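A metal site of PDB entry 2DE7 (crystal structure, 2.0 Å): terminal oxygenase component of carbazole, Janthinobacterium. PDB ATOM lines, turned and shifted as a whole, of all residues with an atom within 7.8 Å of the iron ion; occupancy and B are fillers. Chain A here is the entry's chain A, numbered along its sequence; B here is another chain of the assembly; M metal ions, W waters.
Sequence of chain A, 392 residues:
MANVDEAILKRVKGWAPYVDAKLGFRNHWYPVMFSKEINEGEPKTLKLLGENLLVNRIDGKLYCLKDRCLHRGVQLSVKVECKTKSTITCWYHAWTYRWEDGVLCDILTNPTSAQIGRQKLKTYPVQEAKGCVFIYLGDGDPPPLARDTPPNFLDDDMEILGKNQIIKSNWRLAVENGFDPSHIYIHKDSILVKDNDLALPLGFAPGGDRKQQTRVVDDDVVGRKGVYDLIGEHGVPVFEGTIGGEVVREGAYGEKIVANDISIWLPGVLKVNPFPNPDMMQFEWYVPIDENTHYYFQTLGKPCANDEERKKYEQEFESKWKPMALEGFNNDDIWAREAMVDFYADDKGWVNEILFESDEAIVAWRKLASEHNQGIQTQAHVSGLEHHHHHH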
ATOM      1  N   ASN A 177      17.995 -12.855 -19.902  1.00  0.00           N
ATOM      2  CA  ASN A 177      18.693 -11.862 -20.706  1.00  0.00           C
ATOM      3  C   ASN A 177      19.660 -11.074 -19.836  1.00  0.00           C
ATOM      4  O   ASN A 177      20.785 -10.779 -20.245  1.00  0.00           O
ATOM      5  CB  ASN A 177      17.714 -10.884 -21.356  1.00  0.00           C
ATOM      6  CG  ASN A 177      18.423  -9.772 -22.095  1.00  0.00           C
ATOM      7  OD1 ASN A 177      19.026  -9.996 -23.138  1.00  0.00           O
ATOM      8  ND2 ASN A 177      18.384  -8.564 -21.548  1.00  0.00           N
ATOM      9  N   GLY A 178      19.238 -10.744 -18.625  1.00  0.00           N
ATOM     10  CA  GLY A 178      20.083  -9.982 -17.734  1.00  0.00           C
ATOM     11  C   GLY A 178      21.337 -10.728 -17.301  1.00  0.00           C
ATOM     12  O   GLY A 178      22.416 -10.127 -17.188  1.00  0.00           O
ATOM     13  N   PHE A 179      21.206 -12.030 -17.079  1.00  0.00           N
ATOM     14  CA  PHE A 179      22.335 -12.846 -16.632  1.00  0.00           C
ATOM     15  C   PHE A 179      23.119 -13.479 -17.788  1.00  0.00           C
ATOM     16  O   PHE A 179      24.139 -14.135 -17.572  1.00  0.00           O
ATOM     17  CB  PHE A 179      21.823 -13.923 -15.667  1.00  0.00           C
ATOM     18  CG  PHE A 179      22.915 -14.627 -14.896  1.00  0.00           C
ATOM     19  CD1 PHE A 179      23.845 -13.912 -14.156  1.00  0.00           C
ATOM     20  CD2 PHE A 179      22.973 -16.019 -14.883  1.00  0.00           C
ATOM     21  CE1 PHE A 179      24.837 -14.567 -13.409  1.00  0.00           C
ATOM     22  CE2 PHE A 179      23.957 -16.688 -14.130  1.00  0.00           C
ATOM     23  CZ  PHE A 179      24.882 -15.953 -13.399  1.00  0.00           C
ATOM     24  N   ASP A 180      22.643 -13.273 -19.027  1.00  0.00           N
ATOM     25  CA  ASP A 180      23.247 -13.811 -20.246  1.00  0.00           C
ATOM     26  C   ASP A 180      24.624 -13.178 -20.513  1.00  0.00           C
ATOM     27  O   ASP A 180      24.703 -12.009 -20.888  1.00  0.00           O
ATOM     28  CB  ASP A 180      22.301 -13.519 -21.428  1.00  0.00           C
ATOM     29  CG  ASP A 180      22.676 -14.228 -22.713  1.00  0.00           C
ATOM     30  OD1 ASP A 180      23.883 -14.399 -22.999  1.00  0.00           O
ATOM     31  OD2 ASP A 180      21.739 -14.613 -23.457  1.00  0.00           O
ATOM     32  N   HIS A 183      24.927 -11.604 -24.070  1.00  0.00           N
ATOM     33  CA  HIS A 183      23.967 -10.625 -24.556  1.00  0.00           C
ATOM     34  C   HIS A 183      24.585  -9.229 -24.601  1.00  0.00           C
ATOM     35  O   HIS A 183      24.002  -8.287 -25.123  1.00  0.00           O
ATOM     36  CB  HIS A 183      22.687 -10.610 -23.702  1.00  0.00           C
ATOM     37  CG  HIS A 183      22.697  -9.608 -22.590  1.00  0.00           C
ATOM     38  ND1 HIS A 183      23.384  -9.806 -21.412  1.00  0.00           N
ATOM     39  CD2 HIS A 183      22.105  -8.392 -22.479  1.00  0.00           C
ATOM     40  CE1 HIS A 183      23.207  -8.767 -20.627  1.00  0.00           C
ATOM     41  NE2 HIS A 183      22.437  -7.892 -21.250  1.00  0.00           N
ATOM     42  N   ILE A 184      25.795  -9.119 -24.047  1.00  0.00           N
ATOM     43  CA  ILE A 184      26.556  -7.876 -24.019  1.00  0.00           C
ATOM     44  C   ILE A 184      26.677  -7.306 -25.438  1.00  0.00           C
ATOM     45  O   ILE A 184      26.836  -6.102 -25.635  1.00  0.00           O
ATOM     46  CB  ILE A 184      27.959  -8.132 -23.410  1.00  0.00           C
ATOM     47  CG1 ILE A 184      28.682  -6.826 -23.129  1.00  0.00           C
ATOM     48  CG2 ILE A 184      28.787  -8.991 -24.366  1.00  0.00           C
ATOM     49  CD1 ILE A 184      30.014  -7.040 -22.398  1.00  0.00           C
ATOM     50  N   TYR A 185      26.588  -8.182 -26.429  1.00  0.00           N
ATOM     51  CA  TYR A 185      26.687  -7.782 -27.829  1.00  0.00           C
ATOM     52  C   TYR A 185      25.637  -6.724 -28.213  1.00  0.00           C
ATOM     53  O   TYR A 185      25.893  -5.866 -29.059  1.00  0.00           O
ATOM     54  CB  TYR A 185      26.524  -9.001 -28.737  1.00  0.00           C
ATOM     55  CG  TYR A 185      26.709  -8.726 -30.214  1.00  0.00           C
ATOM     56  CD1 TYR A 185      27.978  -8.563 -30.757  1.00  0.00           C
ATOM     57  CD2 TYR A 185      25.604  -8.614 -31.060  1.00  0.00           C
ATOM     58  CE1 TYR A 185      28.156  -8.295 -32.121  1.00  0.00           C
ATOM     59  CE2 TYR A 185      25.767  -8.341 -32.417  1.00  0.00           C
ATOM     60  CZ  TYR A 185      27.043  -8.188 -32.939  1.00  0.00           C
ATOM     61  OH  TYR A 185      27.207  -7.926 -34.287  1.00  0.00           O
ATOM     62  N   ILE A 186      24.450  -6.783 -27.597  1.00  0.00           N
ATOM     63  CA  ILE A 186      23.397  -5.823 -27.935  1.00  0.00           C
ATOM     64  C   ILE A 186      23.658  -4.426 -27.381  1.00  0.00           C
ATOM     65  O   ILE A 186      22.938  -3.478 -27.723  1.00  0.00           O
ATOM     66  CB  ILE A 186      22.006  -6.257 -27.398  1.00  0.00           C
ATOM     67  CG1 ILE A 186      21.958  -6.096 -25.874  1.00  0.00           C
ATOM     68  CG2 ILE A 186      21.701  -7.687 -27.833  1.00  0.00           C
ATOM     69  CD1 ILE A 186      20.585  -6.376 -25.265  1.00  0.00           C
ATOM     70  N   HIS A 187      24.659  -4.299 -26.520  1.00  0.00           N
ATOM     71  CA  HIS A 187      24.996  -3.014 -25.908  1.00  0.00           C
ATOM     72  C   HIS A 187      26.205  -2.356 -26.572  1.00  0.00           C
ATOM     73  O   HIS A 187      26.672  -1.316 -26.095  1.00  0.00           O
ATOM     74  CB  HIS A 187      25.317  -3.203 -24.418  1.00  0.00           C
ATOM     75  CG  HIS A 187      24.140  -3.641 -23.604  1.00  0.00           C
ATOM     76  ND1 HIS A 187      22.996  -2.893 -23.484  1.00  0.00           N
ATOM     77  CD2 HIS A 187      23.945  -4.750 -22.853  1.00  0.00           C
ATOM     78  CE1 HIS A 187      22.138  -3.518 -22.705  1.00  0.00           C
ATOM     79  NE2 HIS A 187      22.691  -4.650 -22.307  1.00  0.00           N
ATOM     80  N   LEU A 270      19.049  -9.276 -10.354  1.00  0.00           N
ATOM     81  CA  LEU A 270      20.426  -9.268 -10.823  1.00  0.00           C
ATOM     82  C   LEU A 270      21.237  -8.179 -10.136  1.00  0.00           C
ATOM     83  O   LEU A 270      20.734  -7.085  -9.868  1.00  0.00           O
ATOM     84  CB  LEU A 270      20.468  -9.025 -12.340  1.00  0.00           C
ATOM     85  CG  LEU A 270      21.831  -9.078 -13.046  1.00  0.00           C
ATOM     86  CD1 LEU A 270      22.209 -10.530 -13.323  1.00  0.00           C
ATOM     87  CD2 LEU A 270      21.771  -8.302 -14.362  1.00  0.00           C
ATOM     88  N   PHE A 275      28.656  -0.897 -11.539  1.00  0.00           N
ATOM     89  CA  PHE A 275      27.954  -0.457 -12.737  1.00  0.00           C
ATOM     90  C   PHE A 275      26.962   0.639 -12.367  1.00  0.00           C
ATOM     91  O   PHE A 275      26.369   0.587 -11.290  1.00  0.00           O
ATOM     92  CB  PHE A 275      27.197  -1.635 -13.358  1.00  0.00           C
ATOM     93  CG  PHE A 275      26.823  -1.415 -14.796  1.00  0.00           C
ATOM     94  CD1 PHE A 275      27.759  -1.587 -15.812  1.00  0.00           C
ATOM     95  CD2 PHE A 275      25.542  -0.992 -15.140  1.00  0.00           C
ATOM     96  CE1 PHE A 275      27.434  -1.342 -17.135  1.00  0.00           C
ATOM     97  CE2 PHE A 275      25.205  -0.741 -16.466  1.00  0.00           C
ATOM     98  CZ  PHE A 275      26.150  -0.921 -17.470  1.00  0.00           C
ATOM     99  N   GLU A 284      18.748  -5.051 -10.096  1.00  0.00           N
ATOM    100  CA  GLU A 284      17.471  -4.946 -10.806  1.00  0.00           C
ATOM    101  C   GLU A 284      16.621  -6.206 -10.727  1.00  0.00           C
ATOM    102  O   GLU A 284      17.100  -7.311 -10.951  1.00  0.00           O
ATOM    103  CB  GLU A 284      17.690  -4.541 -12.263  1.00  0.00           C
ATOM    104  CG  GLU A 284      18.644  -5.443 -13.059  1.00  0.00           C
ATOM    105  CD  GLU A 284      18.724  -5.027 -14.516  1.00  0.00           C
ATOM    106  OE1 GLU A 284      18.752  -3.807 -14.772  1.00  0.00           O
ATOM    107  OE2 GLU A 284      18.764  -5.901 -15.402  1.00  0.00           O
ATOM    108  N   TYR A 286      13.034  -8.406 -11.828  1.00  0.00           N
ATOM    109  CA  TYR A 286      12.160  -8.688 -12.970  1.00  0.00           C
ATOM    110  C   TYR A 286      10.989  -9.376 -12.257  1.00  0.00           C
ATOM    111  O   TYR A 286      10.932 -10.603 -12.127  1.00  0.00           O
ATOM    112  CB  TYR A 286      12.852  -9.641 -13.952  1.00  0.00           C
ATOM    113  CG  TYR A 286      14.296  -9.281 -14.250  1.00  0.00           C
ATOM    114  CD1 TYR A 286      14.616  -8.187 -15.050  1.00  0.00           C
ATOM    115  CD2 TYR A 286      15.351 -10.022 -13.709  1.00  0.00           C
ATOM    116  CE1 TYR A 286      15.955  -7.846 -15.320  1.00  0.00           C
ATOM    117  CE2 TYR A 286      16.679  -9.697 -13.964  1.00  0.00           C
ATOM    118  CZ  TYR A 286      16.969  -8.603 -14.773  1.00  0.00           C
ATOM    119  OH  TYR A 286      18.286  -8.293 -15.045  1.00  0.00           O
ATOM    120  N   TYR A 296       9.989  -4.016 -14.328  1.00  0.00           N
ATOM    121  CA  TYR A 296      11.434  -3.928 -14.509  1.00  0.00           C
ATOM    122  C   TYR A 296      11.831  -2.883 -13.450  1.00  0.00           C
ATOM    123  O   TYR A 296      11.832  -1.673 -13.716  1.00  0.00           O
ATOM    124  CB  TYR A 296      11.789  -3.472 -15.927  1.00  0.00           C
ATOM    125  CG  TYR A 296      13.279  -3.322 -16.170  1.00  0.00           C
ATOM    126  CD1 TYR A 296      14.206  -4.097 -15.461  1.00  0.00           C
ATOM    127  CD2 TYR A 296      13.772  -2.393 -17.089  1.00  0.00           C
ATOM    128  CE1 TYR A 296      15.587  -3.957 -15.676  1.00  0.00           C
ATOM    129  CE2 TYR A 296      15.141  -2.247 -17.307  1.00  0.00           C
ATOM    130  CZ  TYR A 296      16.047  -3.029 -16.596  1.00  0.00           C
ATOM    131  OH  TYR A 296      17.402  -2.858 -16.771  1.00  0.00           O
ATOM    132  N   PHE A 329      21.305   2.601 -21.524  1.00  0.00           N
ATOM    133  CA  PHE A 329      21.938   1.284 -21.648  1.00  0.00           C
ATOM    134  C   PHE A 329      20.909   0.151 -21.637  1.00  0.00           C
ATOM    135  O   PHE A 329      20.861  -0.659 -22.562  1.00  0.00           O
ATOM    136  CB  PHE A 329      22.933   1.088 -20.511  1.00  0.00           C
ATOM    137  CG  PHE A 329      23.792  -0.154 -20.648  1.00  0.00           C
ATOM    138  CD1 PHE A 329      24.975  -0.124 -21.376  1.00  0.00           C
ATOM    139  CD2 PHE A 329      23.438  -1.341 -20.001  1.00  0.00           C
ATOM    140  CE1 PHE A 329      25.799  -1.242 -21.453  1.00  0.00           C
ATOM    141  CE2 PHE A 329      24.266  -2.468 -20.078  1.00  0.00           C
ATOM    142  CZ  PHE A 329      25.442  -2.420 -20.805  1.00  0.00           C
ATOM    143  N   ASN A 330      20.088   0.110 -20.597  1.00  0.00           N
ATOM    144  CA  ASN A 330      19.104  -0.969 -20.458  1.00  0.00           C
ATOM    145  C   ASN A 330      17.905  -0.953 -21.411  1.00  0.00           C
ATOM    146  O   ASN A 330      17.175  -1.937 -21.475  1.00  0.00           O
ATOM    147  CB  ASN A 330      18.639  -1.050 -18.995  1.00  0.00           C
ATOM    148  CG  ASN A 330      19.767  -1.446 -18.049  1.00  0.00           C
ATOM    149  OD1 ASN A 330      19.993  -0.786 -17.028  1.00  0.00           O
ATOM    150  ND2 ASN A 330      20.474  -2.524 -18.367  1.00  0.00           N
ATOM    151  N   ASN A 331      17.697   0.130 -22.144  1.00  0.00           N
ATOM    152  CA  ASN A 331      16.562   0.126 -23.070  1.00  0.00           C
ATOM    153  C   ASN A 331      16.693  -0.997 -24.105  1.00  0.00           C
ATOM    154  O   ASN A 331      15.684  -1.594 -24.502  1.00  0.00           O
ATOM    155  CB  ASN A 331      16.441   1.477 -23.787  1.00  0.00           C
ATOM    156  CG  ASN A 331      15.579   2.458 -23.013  1.00  0.00           C
ATOM    157  OD1 ASN A 331      14.890   2.084 -22.058  1.00  0.00           O
ATOM    158  ND2 ASN A 331      15.599   3.713 -23.436  1.00  0.00           N
ATOM    159  N   ASP A 332      17.910  -1.287 -24.544  1.00  0.00           N
ATOM    160  CA  ASP A 332      18.086  -2.363 -25.504  1.00  0.00           C
ATOM    161  C   ASP A 332      17.712  -3.707 -24.887  1.00  0.00           C
ATOM    162  O   ASP A 332      17.313  -4.626 -25.610  1.00  0.00           O
ATOM    163  CB  ASP A 332      19.533  -2.401 -26.022  1.00  0.00           C
ATOM    164  CG  ASP A 332      19.849  -1.239 -26.939  1.00  0.00           C
ATOM    165  OD1 ASP A 332      19.068  -1.000 -27.876  1.00  0.00           O
ATOM    166  OD2 ASP A 332      20.878  -0.575 -26.727  1.00  0.00           O
ATOM    167  N   ASP A 333      17.839  -3.835 -23.576  1.00  0.00           N
ATOM    168  CA  ASP A 333      17.480  -5.089 -22.909  1.00  0.00           C
ATOM    169  C   ASP A 333      15.973  -5.297 -23.019  1.00  0.00           C
ATOM    170  O   ASP A 333      15.496  -6.428 -23.164  1.00  0.00           O
ATOM    171  CB  ASP A 333      17.861  -5.073 -21.421  1.00  0.00           C
ATOM    172  CG  ASP A 333      19.348  -5.101 -21.205  1.00  0.00           C
ATOM    173  OD1 ASP A 333      20.012  -6.051 -21.687  1.00  0.00           O
ATOM    174  OD2 ASP A 333      19.867  -4.177 -20.540  1.00  0.00           O
ATOM    175  N   ILE A 334      15.237  -4.188 -22.959  1.00  0.00           N
ATOM    176  CA  ILE A 334      13.788  -4.247 -23.039  1.00  0.00           C
ATOM    177  C   ILE A 334      13.285  -4.864 -24.329  1.00  0.00           C
ATOM    178  O   ILE A 334      12.476  -5.796 -24.293  1.00  0.00           O
ATOM    179  CB  ILE A 334      13.152  -2.837 -22.848  1.00  0.00           C
ATOM    180  CG1 ILE A 334      13.455  -2.323 -21.434  1.00  0.00           C
ATOM    181  CG2 ILE A 334      11.660  -2.895 -23.089  1.00  0.00           C
ATOM    182  CD1 ILE A 334      12.926  -0.929 -21.149  1.00  0.00           C
ATOM    183  N   ALA A 336      14.992  -6.633 -26.360  1.00  0.00           N
ATOM    184  CA  ALA A 336      15.607  -7.944 -26.532  1.00  0.00           C
ATOM    185  C   ALA A 336      14.686  -8.985 -25.869  1.00  0.00           C
ATOM    186  O   ALA A 336      14.448 -10.053 -26.417  1.00  0.00           O
ATOM    187  CB  ALA A 336      16.989  -7.985 -25.896  1.00  0.00           C
ATOM    188  N   ARG A 337      14.179  -8.644 -24.682  1.00  0.00           N
ATOM    189  CA  ARG A 337      13.276  -9.531 -23.948  1.00  0.00           C
ATOM    190  C   ARG A 337      12.003  -9.752 -24.771  1.00  0.00           C
ATOM    191  O   ARG A 337      11.520 -10.875 -24.906  1.00  0.00           O
ATOM    192  CB  ARG A 337      12.858  -8.915 -22.605  1.00  0.00           C
ATOM    193  CG  ARG A 337      14.003  -8.586 -21.668  1.00  0.00           C
ATOM    194  CD  ARG A 337      13.488  -7.865 -20.413  1.00  0.00           C
ATOM    195  NE  ARG A 337      14.573  -7.164 -19.743  1.00  0.00           N
ATOM    196  CZ  ARG A 337      14.402  -6.190 -18.850  1.00  0.00           C
ATOM    197  NH1 ARG A 337      13.174  -5.794 -18.515  1.00  0.00           N
ATOM    198  NH2 ARG A 337      15.450  -5.583 -18.323  1.00  0.00           N
ATOM    199  N   TYR B  92      21.326 -10.427 -31.532  1.00  0.00           N
ATOM    200  CA  TYR B  92      21.368 -10.806 -30.106  1.00  0.00           C
ATOM    201  C   TYR B  92      22.735 -11.308 -29.610  1.00  0.00           C
ATOM    202  O   TYR B  92      23.375 -10.653 -28.790  1.00  0.00           O
ATOM    203  CB  TYR B  92      20.285 -11.861 -29.846  1.00  0.00           C
ATOM    204  CG  TYR B  92      19.726 -11.881 -28.435  1.00  0.00           C
ATOM    205  CD1 TYR B  92      20.308 -11.117 -27.414  1.00  0.00           C
ATOM    206  CD2 TYR B  92      18.628 -12.677 -28.117  1.00  0.00           C
ATOM    207  CE1 TYR B  92      19.795 -11.146 -26.117  1.00  0.00           C
ATOM    208  CE2 TYR B  92      18.109 -12.719 -26.824  1.00  0.00           C
ATOM    209  CZ  TYR B  92      18.688 -11.955 -25.826  1.00  0.00           C
ATOM    210  OH  TYR B  92      18.167 -11.997 -24.555  1.00  0.00           O
HETATM  211 FE    FE M   1      21.784  -6.001 -20.915  1.00  0.00          FE
HETATM  212  O   HOH W   1      22.009  -5.703 -19.072  1.00  0.00           O
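The side-chain carboxylate (OD1) of Asp 333 sits close to the side-chain amide nitrogen (ND2) of Asn 177, 3.0 Å away.
The side-chain carboxylate (OD2) of Asp 333 is in hydrogen-bond range of the side-chain amide nitrogen (ND2) of Asn 330 (2.8 Å).
O of Asn 177 is in hydrogen-bond range of ND1 of His 183 (3.0 Å).
A ring nitrogen (ND1) of His 183 sits at hydrogen-bond distance from the backbone carbonyl oxygen (O) of Asp 180 (2.6 Å).
A ring nitrogen (ND1) of His 187 sits close to the backbone carbonyl oxygen (O) of Phe 329, 3.2 Å away.
The iron ion is bound by water W1, OD1 of Asp 333, NE2 of His 183 and NE2 of His 187.
The iron ion has four donor atoms within binding distance.
Slightly farther from the iron ion lies OD2 of Asp 333 (2.7 Å).
Of the 23 residues printed, 3 come within 4 Å of the iron ion.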
